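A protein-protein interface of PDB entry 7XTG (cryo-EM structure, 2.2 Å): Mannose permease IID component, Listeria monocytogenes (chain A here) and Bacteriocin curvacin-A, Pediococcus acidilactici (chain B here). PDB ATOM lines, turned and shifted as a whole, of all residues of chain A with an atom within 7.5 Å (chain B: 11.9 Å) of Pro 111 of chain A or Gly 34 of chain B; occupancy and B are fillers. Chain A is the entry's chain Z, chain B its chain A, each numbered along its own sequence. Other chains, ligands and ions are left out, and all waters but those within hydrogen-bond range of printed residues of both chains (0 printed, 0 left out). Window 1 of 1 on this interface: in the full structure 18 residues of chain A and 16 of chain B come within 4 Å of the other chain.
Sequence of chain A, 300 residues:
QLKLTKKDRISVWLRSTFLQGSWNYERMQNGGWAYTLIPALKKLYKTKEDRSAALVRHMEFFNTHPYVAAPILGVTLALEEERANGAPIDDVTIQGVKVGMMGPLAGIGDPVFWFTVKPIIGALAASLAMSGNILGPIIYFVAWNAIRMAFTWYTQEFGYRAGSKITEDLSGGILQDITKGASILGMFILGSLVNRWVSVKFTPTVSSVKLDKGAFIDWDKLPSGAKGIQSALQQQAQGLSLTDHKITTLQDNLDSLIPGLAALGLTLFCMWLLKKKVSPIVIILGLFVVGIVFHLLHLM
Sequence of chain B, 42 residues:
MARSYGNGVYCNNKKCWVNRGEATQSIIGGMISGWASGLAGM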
ATOM      1  N   HIS A  65     -10.239   6.615  -4.207  1.00  0.00           N
ATOM      2  CA  HIS A  65     -10.144   6.705  -5.655  1.00  0.00           C
ATOM      3  C   HIS A  65     -11.432   6.151  -6.260  1.00  0.00           C
ATOM      4  O   HIS A  65     -11.829   5.025  -5.926  1.00  0.00           O
ATOM      5  CB  HIS A  65      -8.920   5.946  -6.163  1.00  0.00           C
ATOM      6  CG  HIS A  65      -8.834   5.870  -7.653  1.00  0.00           C
ATOM      7  ND1 HIS A  65      -7.990   6.671  -8.389  1.00  0.00           N
ATOM      8  CD2 HIS A  65      -9.477   5.081  -8.544  1.00  0.00           C
ATOM      9  CE1 HIS A  65      -8.126   6.386  -9.672  1.00  0.00           C
ATOM     10  NE2 HIS A  65      -9.022   5.425  -9.793  1.00  0.00           N
ATOM     11  N   PRO A 104      -6.709   2.029   2.364  1.00  0.00           N
ATOM     12  CA  PRO A 104      -5.758   1.209   1.599  1.00  0.00           C
ATOM     13  C   PRO A 104      -6.090   1.097   0.124  1.00  0.00           C
ATOM     14  O   PRO A 104      -5.175   1.066  -0.708  1.00  0.00           O
ATOM     15  CB  PRO A 104      -5.860  -0.137   2.330  1.00  0.00           C
ATOM     16  CG  PRO A 104      -6.027   0.341   3.745  1.00  0.00           C
ATOM     17  CD  PRO A 104      -7.213   1.236   3.498  1.00  0.00           C
ATOM     18  N   LEU A 105      -7.375   1.043  -0.234  1.00  0.00           N
ATOM     19  CA  LEU A 105      -7.720   0.987  -1.649  1.00  0.00           C
ATOM     20  C   LEU A 105      -7.393   2.297  -2.352  1.00  0.00           C
ATOM     21  O   LEU A 105      -6.979   2.289  -3.514  1.00  0.00           O
ATOM     22  CB  LEU A 105      -9.188   0.616  -1.835  1.00  0.00           C
ATOM     23  CG  LEU A 105      -9.495  -0.858  -1.575  1.00  0.00           C
ATOM     24  CD1 LEU A 105     -10.907  -1.160  -2.012  1.00  0.00           C
ATOM     25  CD2 LEU A 105      -8.499  -1.761  -2.299  1.00  0.00           C
ATOM     26  N   ALA A 106      -7.558   3.435  -1.673  1.00  0.00           N
ATOM     27  CA  ALA A 106      -7.122   4.696  -2.265  1.00  0.00           C
ATOM     28  C   ALA A 106      -5.611   4.711  -2.466  1.00  0.00           C
ATOM     29  O   ALA A 106      -5.121   5.146  -3.516  1.00  0.00           O
ATOM     30  CB  ALA A 106      -7.563   5.873  -1.398  1.00  0.00           C
ATOM     31  N   GLY A 107      -4.857   4.236  -1.471  1.00  0.00           N
ATOM     32  CA  GLY A 107      -3.408   4.187  -1.587  1.00  0.00           C
ATOM     33  C   GLY A 107      -2.895   3.174  -2.591  1.00  0.00           C
ATOM     34  O   GLY A 107      -1.742   3.273  -3.019  1.00  0.00           O
ATOM     35  N   ILE A 108      -3.714   2.190  -2.949  1.00  0.00           N
ATOM     36  CA  ILE A 108      -3.327   1.249  -3.994  1.00  0.00           C
ATOM     37  C   ILE A 108      -3.881   1.665  -5.361  1.00  0.00           C
ATOM     38  O   ILE A 108      -3.400   1.188  -6.393  1.00  0.00           O
ATOM     39  CB  ILE A 108      -3.773  -0.175  -3.614  1.00  0.00           C
ATOM     40  CG1 ILE A 108      -2.934  -1.228  -4.340  1.00  0.00           C
ATOM     41  CG2 ILE A 108      -5.238  -0.379  -3.919  1.00  0.00           C
ATOM     42  CD1 ILE A 108      -1.446  -1.071  -4.130  1.00  0.00           C
ATOM     43  N   GLY A 109      -4.873   2.552  -5.394  1.00  0.00           N
ATOM     44  CA  GLY A 109      -5.465   2.984  -6.642  1.00  0.00           C
ATOM     45  C   GLY A 109      -4.820   4.225  -7.217  1.00  0.00           C
ATOM     46  O   GLY A 109      -4.638   4.321  -8.434  1.00  0.00           O
ATOM     47  N   ASP A 110      -4.472   5.185  -6.355  1.00  0.00           N
ATOM     48  CA  ASP A 110      -3.789   6.391  -6.822  1.00  0.00           C
ATOM     49  C   ASP A 110      -2.531   6.072  -7.620  1.00  0.00           C
ATOM     50  O   ASP A 110      -2.304   6.721  -8.654  1.00  0.00           O
ATOM     51  CB  ASP A 110      -3.489   7.312  -5.633  1.00  0.00           C
ATOM     52  CG  ASP A 110      -4.652   8.229  -5.296  1.00  0.00           C
ATOM     53  OD1 ASP A 110      -5.799   7.897  -5.659  1.00  0.00           O
ATOM     54  OD2 ASP A 110      -4.410   9.282  -4.668  1.00  0.00           O
ATOM     55  N   PRO A 111      -1.683   5.119  -7.225  1.00  0.00           N
ATOM     56  CA  PRO A 111      -0.589   4.735  -8.128  1.00  0.00           C
ATOM     57  C   PRO A 111      -1.061   4.039  -9.394  1.00  0.00           C
ATOM     58  O   PRO A 111      -0.654   4.440 -10.491  1.00  0.00           O
ATOM     59  CB  PRO A 111       0.275   3.810  -7.259  1.00  0.00           C
ATOM     60  CG  PRO A 111      -0.614   3.354  -6.162  1.00  0.00           C
ATOM     61  CD  PRO A 111      -1.532   4.498  -5.897  1.00  0.00           C
ATOM     62  N   VAL A 112      -1.927   3.028  -9.280  1.00  0.00           N
ATOM     63  CA  VAL A 112      -2.250   2.182 -10.428  1.00  0.00           C
ATOM     64  C   VAL A 112      -2.914   2.991 -11.536  1.00  0.00           C
ATOM     65  O   VAL A 112      -2.514   2.917 -12.704  1.00  0.00           O
ATOM     66  CB  VAL A 112      -3.141   1.004  -9.991  1.00  0.00           C
ATOM     67  CG1 VAL A 112      -3.837   0.377 -11.195  1.00  0.00           C
ATOM     68  CG2 VAL A 112      -2.320  -0.032  -9.240  1.00  0.00           C
ATOM     69  N   PHE A 113      -3.933   3.776 -11.194  1.00  0.00           N
ATOM     70  CA  PHE A 113      -4.737   4.452 -12.206  1.00  0.00           C
ATOM     71  C   PHE A 113      -4.222   5.848 -12.543  1.00  0.00           C
ATOM     72  O   PHE A 113      -4.166   6.208 -13.719  1.00  0.00           O
ATOM     73  CB  PHE A 113      -6.204   4.515 -11.761  1.00  0.00           C
ATOM     74  CG  PHE A 113      -6.887   3.170 -11.729  1.00  0.00           C
ATOM     75  CD1 PHE A 113      -7.595   2.709 -12.831  1.00  0.00           C
ATOM     76  CD2 PHE A 113      -6.812   2.368 -10.603  1.00  0.00           C
ATOM     77  CE1 PHE A 113      -8.226   1.476 -12.806  1.00  0.00           C
ATOM     78  CE2 PHE A 113      -7.436   1.131 -10.572  1.00  0.00           C
ATOM     79  CZ  PHE A 113      -8.142   0.686 -11.674  1.00  0.00           C
ATOM     80  N   TRP A 114      -3.829   6.637 -11.535  1.00  0.00           N
ATOM     81  CA  TRP A 114      -3.389   8.010 -11.784  1.00  0.00           C
ATOM     82  C   TRP A 114      -1.967   8.096 -12.325  1.00  0.00           C
ATOM     83  O   TRP A 114      -1.754   8.653 -13.408  1.00  0.00           O
ATOM     84  CB  TRP A 114      -3.455   8.850 -10.506  1.00  0.00           C
ATOM     85  CG  TRP A 114      -4.815   9.113  -9.912  1.00  0.00           C
ATOM     86  CD1 TRP A 114      -5.102   9.233  -8.584  1.00  0.00           C
ATOM     87  CD2 TRP A 114      -6.050   9.359 -10.610  1.00  0.00           C
ATOM     88  NE1 TRP A 114      -6.436   9.495  -8.407  1.00  0.00           N
ATOM     89  CE2 TRP A 114      -7.040   9.580  -9.633  1.00  0.00           C
ATOM     90  CE3 TRP A 114      -6.417   9.395 -11.960  1.00  0.00           C
ATOM     91  CZ2 TRP A 114      -8.366   9.836  -9.959  1.00  0.00           C
ATOM     92  CZ3 TRP A 114      -7.739   9.641 -12.282  1.00  0.00           C
ATOM     93  CH2 TRP A 114      -8.696   9.863 -11.285  1.00  0.00           C
ATOM     94  N   PHE A 115      -0.985   7.578 -11.584  1.00  0.00           N
ATOM     95  CA  PHE A 115       0.419   7.848 -11.852  1.00  0.00           C
ATOM     96  C   PHE A 115       1.153   6.726 -12.573  1.00  0.00           C
ATOM     97  O   PHE A 115       2.365   6.851 -12.787  1.00  0.00           O
ATOM     98  CB  PHE A 115       1.159   8.149 -10.535  1.00  0.00           C
ATOM     99  CG  PHE A 115       0.635   9.355  -9.793  1.00  0.00           C
ATOM    100  CD1 PHE A 115       0.819  10.638 -10.289  1.00  0.00           C
ATOM    101  CD2 PHE A 115      -0.067   9.196  -8.609  1.00  0.00           C
ATOM    102  CE1 PHE A 115       0.336  11.735  -9.600  1.00  0.00           C
ATOM    103  CE2 PHE A 115      -0.556  10.288  -7.924  1.00  0.00           C
ATOM    104  CZ  PHE A 115      -0.358  11.557  -8.416  1.00  0.00           C
ATOM    105  N   THR A 116       0.479   5.631 -12.925  1.00  0.00           N
ATOM    106  CA  THR A 116       1.119   4.531 -13.639  1.00  0.00           C
ATOM    107  C   THR A 116       0.495   4.271 -15.004  1.00  0.00           C
ATOM    108  O   THR A 116       1.211   4.270 -16.008  1.00  0.00           O
ATOM    109  CB  THR A 116       1.085   3.260 -12.783  1.00  0.00           C
ATOM    110  OG1 THR A 116       1.776   3.502 -11.551  1.00  0.00           O
ATOM    111  CG2 THR A 116       1.727   2.102 -13.523  1.00  0.00           C
ATOM    112  N   VAL A 117      -0.821   4.062 -15.079  1.00  0.00           N
ATOM    113  CA  VAL A 117      -1.452   3.701 -16.348  1.00  0.00           C
ATOM    114  C   VAL A 117      -1.916   4.941 -17.112  1.00  0.00           C
ATOM    115  O   VAL A 117      -1.772   5.020 -18.342  1.00  0.00           O
ATOM    116  CB  VAL A 117      -2.591   2.686 -16.106  1.00  0.00           C
ATOM    117  CG1 VAL A 117      -3.867   3.362 -15.638  1.00  0.00           C
ATOM    118  CG2 VAL A 117      -2.862   1.884 -17.370  1.00  0.00           C
ATOM    119  N   LYS A 118      -2.471   5.930 -16.402  1.00  0.00           N
ATOM    120  CA  LYS A 118      -2.925   7.146 -17.074  1.00  0.00           C
ATOM    121  C   LYS A 118      -1.806   7.864 -17.815  1.00  0.00           C
ATOM    122  O   LYS A 118      -2.004   8.207 -18.992  1.00  0.00           O
ATOM    123  CB  LYS A 118      -3.600   8.085 -16.070  1.00  0.00           C
ATOM    124  CG  LYS A 118      -4.040   9.391 -16.682  1.00  0.00           C
ATOM    125  CD  LYS A 118      -4.676  10.301 -15.655  1.00  0.00           C
ATOM    126  CE  LYS A 118      -3.695  11.377 -15.223  1.00  0.00           C
ATOM    127  NZ  LYS A 118      -3.455  12.375 -16.301  1.00  0.00           N
ATOM    128  N   PRO A 119      -0.631   8.125 -17.220  1.00  0.00           N
ATOM    129  CA  PRO A 119       0.419   8.811 -17.984  1.00  0.00           C
ATOM    130  C   PRO A 119       0.980   8.017 -19.156  1.00  0.00           C
ATOM    131  O   PRO A 119       1.355   8.629 -20.153  1.00  0.00           O
ATOM    132  CB  PRO A 119       1.438   9.094 -16.855  1.00  0.00           C
ATOM    133  CG  PRO A 119       0.599   8.471 -15.640  1.00  0.00           C
ATOM    134  CD  PRO A 119       0.181   7.357 -16.236  1.00  0.00           C
ATOM    135  N   ILE A 189      13.572   8.886  -3.228  1.00  0.00           N
ATOM    136  CA  ILE A 189      13.265   9.261  -4.600  1.00  0.00           C
ATOM    137  C   ILE A 189      12.864  10.725  -4.678  1.00  0.00           C
ATOM    138  O   ILE A 189      13.096  11.381  -5.696  1.00  0.00           O
ATOM    139  CB  ILE A 189      12.185   8.337  -5.193  1.00  0.00           C
ATOM    140  CG1 ILE A 189      12.452   8.129  -6.680  1.00  0.00           C
ATOM    141  CG2 ILE A 189      10.791   8.914  -5.006  1.00  0.00           C
ATOM    142  CD1 ILE A 189      13.621   7.221  -6.947  1.00  0.00           C
ATOM    143  N   LEU A 193      14.483  13.522  -7.011  1.00  0.00           N
ATOM    144  CA  LEU A 193      13.671  14.385  -7.862  1.00  0.00           C
ATOM    145  C   LEU A 193      13.847  15.858  -7.519  1.00  0.00           C
ATOM    146  O   LEU A 193      13.743  16.710  -8.404  1.00  0.00           O
ATOM    147  CB  LEU A 193      12.197  14.001  -7.763  1.00  0.00           C
ATOM    148  CG  LEU A 193      11.780  12.613  -8.250  1.00  0.00           C
ATOM    149  CD1 LEU A 193      10.304  12.397  -7.971  1.00  0.00           C
ATOM    150  CD2 LEU A 193      12.083  12.453  -9.724  1.00  0.00           C
ATOM    151  N   GLN B  25      11.879   9.580 -18.590  1.00  0.00           N
ATOM    152  CA  GLN B  25      12.344   9.799 -17.223  1.00  0.00           C
ATOM    153  C   GLN B  25      11.228  10.357 -16.351  1.00  0.00           C
ATOM    154  O   GLN B  25      11.053   9.929 -15.204  1.00  0.00           O
ATOM    155  CB  GLN B  25      13.554  10.738 -17.200  1.00  0.00           C
ATOM    156  CG  GLN B  25      14.787  10.299 -17.999  1.00  0.00           C
ATOM    157  CD  GLN B  25      14.780   8.829 -18.392  1.00  0.00           C
ATOM    158  OE1 GLN B  25      15.071   7.952 -17.575  1.00  0.00           O
ATOM    159  NE2 GLN B  25      14.463   8.555 -19.655  1.00  0.00           N
ATOM    160  N   SER B  26      10.464  11.317 -16.874  1.00  0.00           N
ATOM    161  CA  SER B  26       9.366  11.882 -16.103  1.00  0.00           C
ATOM    162  C   SER B  26       8.295  10.840 -15.814  1.00  0.00           C
ATOM    163  O   SER B  26       7.756  10.798 -14.704  1.00  0.00           O
ATOM    164  CB  SER B  26       8.774  13.089 -16.827  1.00  0.00           C
ATOM    165  OG  SER B  26       9.745  14.106 -17.002  1.00  0.00           O
ATOM    166  N   ILE B  27       7.979   9.980 -16.785  1.00  0.00           N
ATOM    167  CA  ILE B  27       6.947   8.977 -16.537  1.00  0.00           C
ATOM    168  C   ILE B  27       7.412   7.986 -15.473  1.00  0.00           C
ATOM    169  O   ILE B  27       6.645   7.615 -14.575  1.00  0.00           O
ATOM    170  CB  ILE B  27       6.525   8.287 -17.852  1.00  0.00           C
ATOM    171  CG1 ILE B  27       5.117   7.713 -17.733  1.00  0.00           C
ATOM    172  CG2 ILE B  27       7.465   7.167 -18.256  1.00  0.00           C
ATOM    173  CD1 ILE B  27       4.311   7.929 -18.976  1.00  0.00           C
ATOM    174  N   ILE B  28       8.688   7.588 -15.512  1.00  0.00           N
ATOM    175  CA  ILE B  28       9.181   6.627 -14.526  1.00  0.00           C
ATOM    176  C   ILE B  28       9.245   7.259 -13.136  1.00  0.00           C
ATOM    177  O   ILE B  28       8.860   6.638 -12.134  1.00  0.00           O
ATOM    178  CB  ILE B  28      10.541   6.053 -14.969  1.00  0.00           C
ATOM    179  CG1 ILE B  28      10.321   4.926 -15.986  1.00  0.00           C
ATOM    180  CG2 ILE B  28      11.352   5.587 -13.769  1.00  0.00           C
ATOM    181  CD1 ILE B  28      11.532   4.583 -16.811  1.00  0.00           C
ATOM    182  N   GLY B  29       9.723   8.503 -13.051  1.00  0.00           N
ATOM    183  CA  GLY B  29       9.765   9.183 -11.767  1.00  0.00           C
ATOM    184  C   GLY B  29       8.388   9.446 -11.192  1.00  0.00           C
ATOM    185  O   GLY B  29       8.179   9.330  -9.982  1.00  0.00           O
ATOM    186  N   GLY B  30       7.429   9.810 -12.046  1.00  0.00           N
ATOM    187  CA  GLY B  30       6.062   9.952 -11.582  1.00  0.00           C
ATOM    188  C   GLY B  30       5.495   8.642 -11.082  1.00  0.00           C
ATOM    189  O   GLY B  30       4.787   8.605 -10.075  1.00  0.00           O
ATOM    190  N   MET B  31       5.802   7.547 -11.779  1.00  0.00           N
ATOM    191  CA  MET B  31       5.365   6.234 -11.322  1.00  0.00           C
ATOM    192  C   MET B  31       5.902   5.936  -9.927  1.00  0.00           C
ATOM    193  O   MET B  31       5.148   5.540  -9.025  1.00  0.00           O
ATOM    194  CB  MET B  31       5.817   5.166 -12.315  1.00  0.00           C
ATOM    195  CG  MET B  31       4.780   4.105 -12.597  1.00  0.00           C
ATOM    196  SD  MET B  31       4.818   2.844 -11.311  1.00  0.00           S
ATOM    197  CE  MET B  31       6.537   2.344 -11.362  1.00  0.00           C
ATOM    198  N   ILE B  32       7.206   6.150  -9.725  1.00  0.00           N
ATOM    199  CA  ILE B  32       7.812   5.870  -8.424  1.00  0.00           C
ATOM    200  C   ILE B  32       7.204   6.759  -7.347  1.00  0.00           C
ATOM    201  O   ILE B  32       6.862   6.293  -6.251  1.00  0.00           O
ATOM    202  CB  ILE B  32       9.340   6.040  -8.491  1.00  0.00           C
ATOM    203  CG1 ILE B  32       9.938   5.104  -9.538  1.00  0.00           C
ATOM    204  CG2 ILE B  32       9.956   5.753  -7.136  1.00  0.00           C
ATOM    205  CD1 ILE B  32      11.347   5.484  -9.959  1.00  0.00           C
ATOM    206  N   SER B  33       7.068   8.057  -7.637  1.00  0.00           N
ATOM    207  CA  SER B  33       6.566   8.990  -6.634  1.00  0.00           C
ATOM    208  C   SER B  33       5.130   8.666  -6.254  1.00  0.00           C
ATOM    209  O   SER B  33       4.787   8.630  -5.067  1.00  0.00           O
ATOM    210  CB  SER B  33       6.666  10.424  -7.153  1.00  0.00           C
ATOM    211  OG  SER B  33       7.811  10.603  -7.961  1.00  0.00           O
ATOM    212  N   GLY B  34       4.274   8.427  -7.248  1.00  0.00           N
ATOM    213  CA  GLY B  34       2.895   8.092  -6.955  1.00  0.00           C
ATOM    214  C   GLY B  34       2.768   6.806  -6.165  1.00  0.00           C
ATOM    215  O   GLY B  34       1.998   6.738  -5.205  1.00  0.00           O
ATOM    216  N   TRP B  35       3.537   5.779  -6.536  1.00  0.00           N
ATOM    217  CA  TRP B  35       3.458   4.518  -5.808  1.00  0.00           C
ATOM    218  C   TRP B  35       3.902   4.690  -4.362  1.00  0.00           C
ATOM    219  O   TRP B  35       3.204   4.268  -3.431  1.00  0.00           O
ATOM    220  CB  TRP B  35       4.297   3.462  -6.519  1.00  0.00           C
ATOM    221  CG  TRP B  35       3.474   2.400  -7.174  1.00  0.00           C
ATOM    222  CD1 TRP B  35       3.157   2.315  -8.497  1.00  0.00           C
ATOM    223  CD2 TRP B  35       2.868   1.264  -6.544  1.00  0.00           C
ATOM    224  NE1 TRP B  35       2.388   1.200  -8.733  1.00  0.00           N
ATOM    225  CE2 TRP B  35       2.200   0.536  -7.550  1.00  0.00           C
ATOM    226  CE3 TRP B  35       2.822   0.793  -5.227  1.00  0.00           C
ATOM    227  CZ2 TRP B  35       1.495  -0.634  -7.281  1.00  0.00           C
ATOM    228  CZ3 TRP B  35       2.122  -0.370  -4.961  1.00  0.00           C
ATOM    229  CH2 TRP B  35       1.472  -1.073  -5.984  1.00  0.00           C
ATOM    230  N   ALA B  36       5.055   5.330  -4.150  1.00  0.00           N
ATOM    231  CA  ALA B  36       5.573   5.490  -2.795  1.00  0.00           C
ATOM    232  C   ALA B  36       4.639   6.338  -1.941  1.00  0.00           C
ATOM    233  O   ALA B  36       4.370   6.005  -0.782  1.00  0.00           O
ATOM    234  CB  ALA B  36       6.972   6.103  -2.837  1.00  0.00           C
ATOM    235  N   SER B  37       4.131   7.440  -2.498  1.00  0.00           N
ATOM    236  CA  SER B  37       3.232   8.302  -1.741  1.00  0.00           C
ATOM    237  C   SER B  37       1.915   7.606  -1.427  1.00  0.00           C
ATOM    238  O   SER B  37       1.403   7.733  -0.313  1.00  0.00           O
ATOM    239  CB  SER B  37       2.989   9.603  -2.500  1.00  0.00           C
ATOM    240  OG  SER B  37       2.960   9.375  -3.898  1.00  0.00           O
ATOM    241  N   GLY B  38       1.338   6.882  -2.389  1.00  0.00           N
ATOM    242  CA  GLY B  38       0.113   6.155  -2.107  1.00  0.00           C
ATOM    243  C   GLY B  38       0.310   5.068  -1.070  1.00  0.00           C
ATOM    244  O   GLY B  38      -0.570   4.810  -0.246  1.00  0.00           O
ATOM    245  N   LEU B  39       1.477   4.421  -1.088  1.00  0.00           N
ATOM    246  CA  LEU B  39       1.752   3.378  -0.109  1.00  0.00           C
ATOM    247  C   LEU B  39       1.993   3.960   1.279  1.00  0.00           C
ATOM    248  O   LEU B  39       1.580   3.364   2.280  1.00  0.00           O
ATOM    249  CB  LEU B  39       2.950   2.548  -0.568  1.00  0.00           C
ATOM    250  CG  LEU B  39       2.676   1.543  -1.685  1.00  0.00           C
ATOM    251  CD1 LEU B  39       3.847   0.592  -1.839  1.00  0.00           C
ATOM    252  CD2 LEU B  39       1.387   0.772  -1.427  1.00  0.00           C
ATOM    253  N   ALA B  40       2.654   5.117   1.362  1.00  0.00           N
ATOM    254  CA  ALA B  40       2.937   5.737   2.652  1.00  0.00           C
ATOM    255  C   ALA B  40       1.731   6.470   3.231  1.00  0.00           C
ATOM    256  O   ALA B  40       1.575   6.521   4.456  1.00  0.00           O
ATOM    257  CB  ALA B  40       4.119   6.699   2.522  1.00  0.00           C
ATOM    258  N   GLY B  41       0.881   7.048   2.380  1.00  0.00           N
ATOM    259  CA  GLY B  41      -0.234   7.837   2.877  1.00  0.00           C
ATOM    260  C   GLY B  41      -1.229   7.012   3.666  1.00  0.00           C
ATOM    261  O   GLY B  41      -1.954   7.540   4.511  1.00  0.00           O
ATOM    262  N   MET B  42      -1.282   5.715   3.398  1.00  0.00           N
ATOM    263  CA  MET B  42      -2.171   4.800   4.101  1.00  0.00           C
ATOM    264  C   MET B  42      -1.527   4.244   5.371  1.00  0.00           C
ATOM    265  O   MET B  42      -2.209   4.008   6.372  1.00  0.00           O
ATOM    266  CB  MET B  42      -2.591   3.670   3.154  1.00  0.00           C
ATOM    267  CG  MET B  42      -3.015   2.389   3.828  1.00  0.00           C
ATOM    268  SD  MET B  42      -1.606   1.294   4.109  1.00  0.00           S
ATOM    269  CE  MET B  42      -0.839   1.298   2.491  1.00  0.00           C
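The backbone carbonyl oxygen (O) of Gly 29 of chain B is in hydrogen-bond range of the side-chain hydroxyl (OG) of Ser 33 of chain B, 2.4 Å away.
The side-chain hydroxyl (OG) of Ser 37 of chain B lies within hydrogen-bond range of the backbone carbonyl oxygen (O) of Gly 34 of chain B.
The backbone carbonyl oxygen (O) of Asp 110 of chain A is in hydrogen-bond range of the backbone NH (N) of Phe 115 of chain A, 3.3 Å away.
The backbone carbonyl oxygen (O) of Pro 111 of chain A is in hydrogen-bond range of the side-chain hydroxyl (OG1) of Thr 116 of chain A, at 2.8 Å.
No residue of chain B comes within 4 Å of Ala 106 of chain A.
Of chain B, only Gly 38 and Leu 39 come within 4 Å of Gly 107 of chain A.
No residue of chain B comes within 4 Å of Asp 110 of chain A.
Of the printed residues of chain B, Pro 111 of chain A touches Gly 34 and Trp 35.
Phe 115 of chain A touches just these residues of chain B: Gly 30, Met 31 and Gly 34.
Thr 116 of chain A touches just these residues of chain B: Met 31 and Trp 35.
Of the printed residues of chain A, Met 31 of chain B touches Phe 115 (3.4 Å) and Thr 116 (3.1 Å).
Gly 34 of chain B touches just these residues of chain A: Pro 111 and Phe 115.
Ser 37 of chain B touches none of the printed residues of chain A.
Printed residues of chain A within 4 Å of Met 42 of chain B: Pro 104 (3.6 Å).
The nearest residue of chain A that does not touch Gly 34 of chain B is Asp 110 of chain A (5.2 Å).
The nearest printed residue of chain A that does not touch Leu 39 of chain B is Ile 108 of chain A (4.3 Å).
Of the 18 printed residues of chain B, 10 touch a printed residue of chain A.
Hydrophobic or aromatic side chains of chain B within 4 Å of the printed part of chain A: Ile 27, Met 31, Ile 32, Trp 35 and Met 42.
Of the 19 printed residues of chain A, 9 touch a printed residue of chain B.
Along chain A the printed residues that touch a printed residue of chain B span positions 104 to 193.
Among the printed residues, no Asp or Glu carboxylate lies within 4 Å of a Lys or Arg side-chain nitrogen of the other chain.
The side-chain sulfur (SD) of Met 31 of chain B lies within hydrogen-bond range of the side-chain hydroxyl (OG1) of Thr 116 of chain A (3.1 Å).
O of Gly 107 of chain A sits close to O of Gly 38 of chain B (3.4 Å).
Met 42 of chain B touches Pro 104 of chain A (CG to CG, 3.6 Å).
Gly 107 of chain A touches Leu 39 of chain B (O to N, 3.9 Å).
Ile 108 of chain A touches Trp 35 of chain B.
CB of Pro 111 of chain A touches O of Gly 34 of chain B, at 3.97 Å.
Trp 35 of chain B touches Pro 111 of chain A (CD1 to CB, 3.5 Å).
O of Gly 30 of chain B touches CB of Phe 115 of chain A, 3.7 Å away.
Met 31 of chain B touches Phe 115 of chain A (CA to O, 3.4 Å).
Phe 115 of chain A touches Gly 34 of chain B.
Pro 119 of chain A touches Ile 27 of chain B (O to CD1, 3.3 Å).
CD1 of Leu 193 of chain A touches OG of Ser 33 of chain B, 3.1 Å away.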
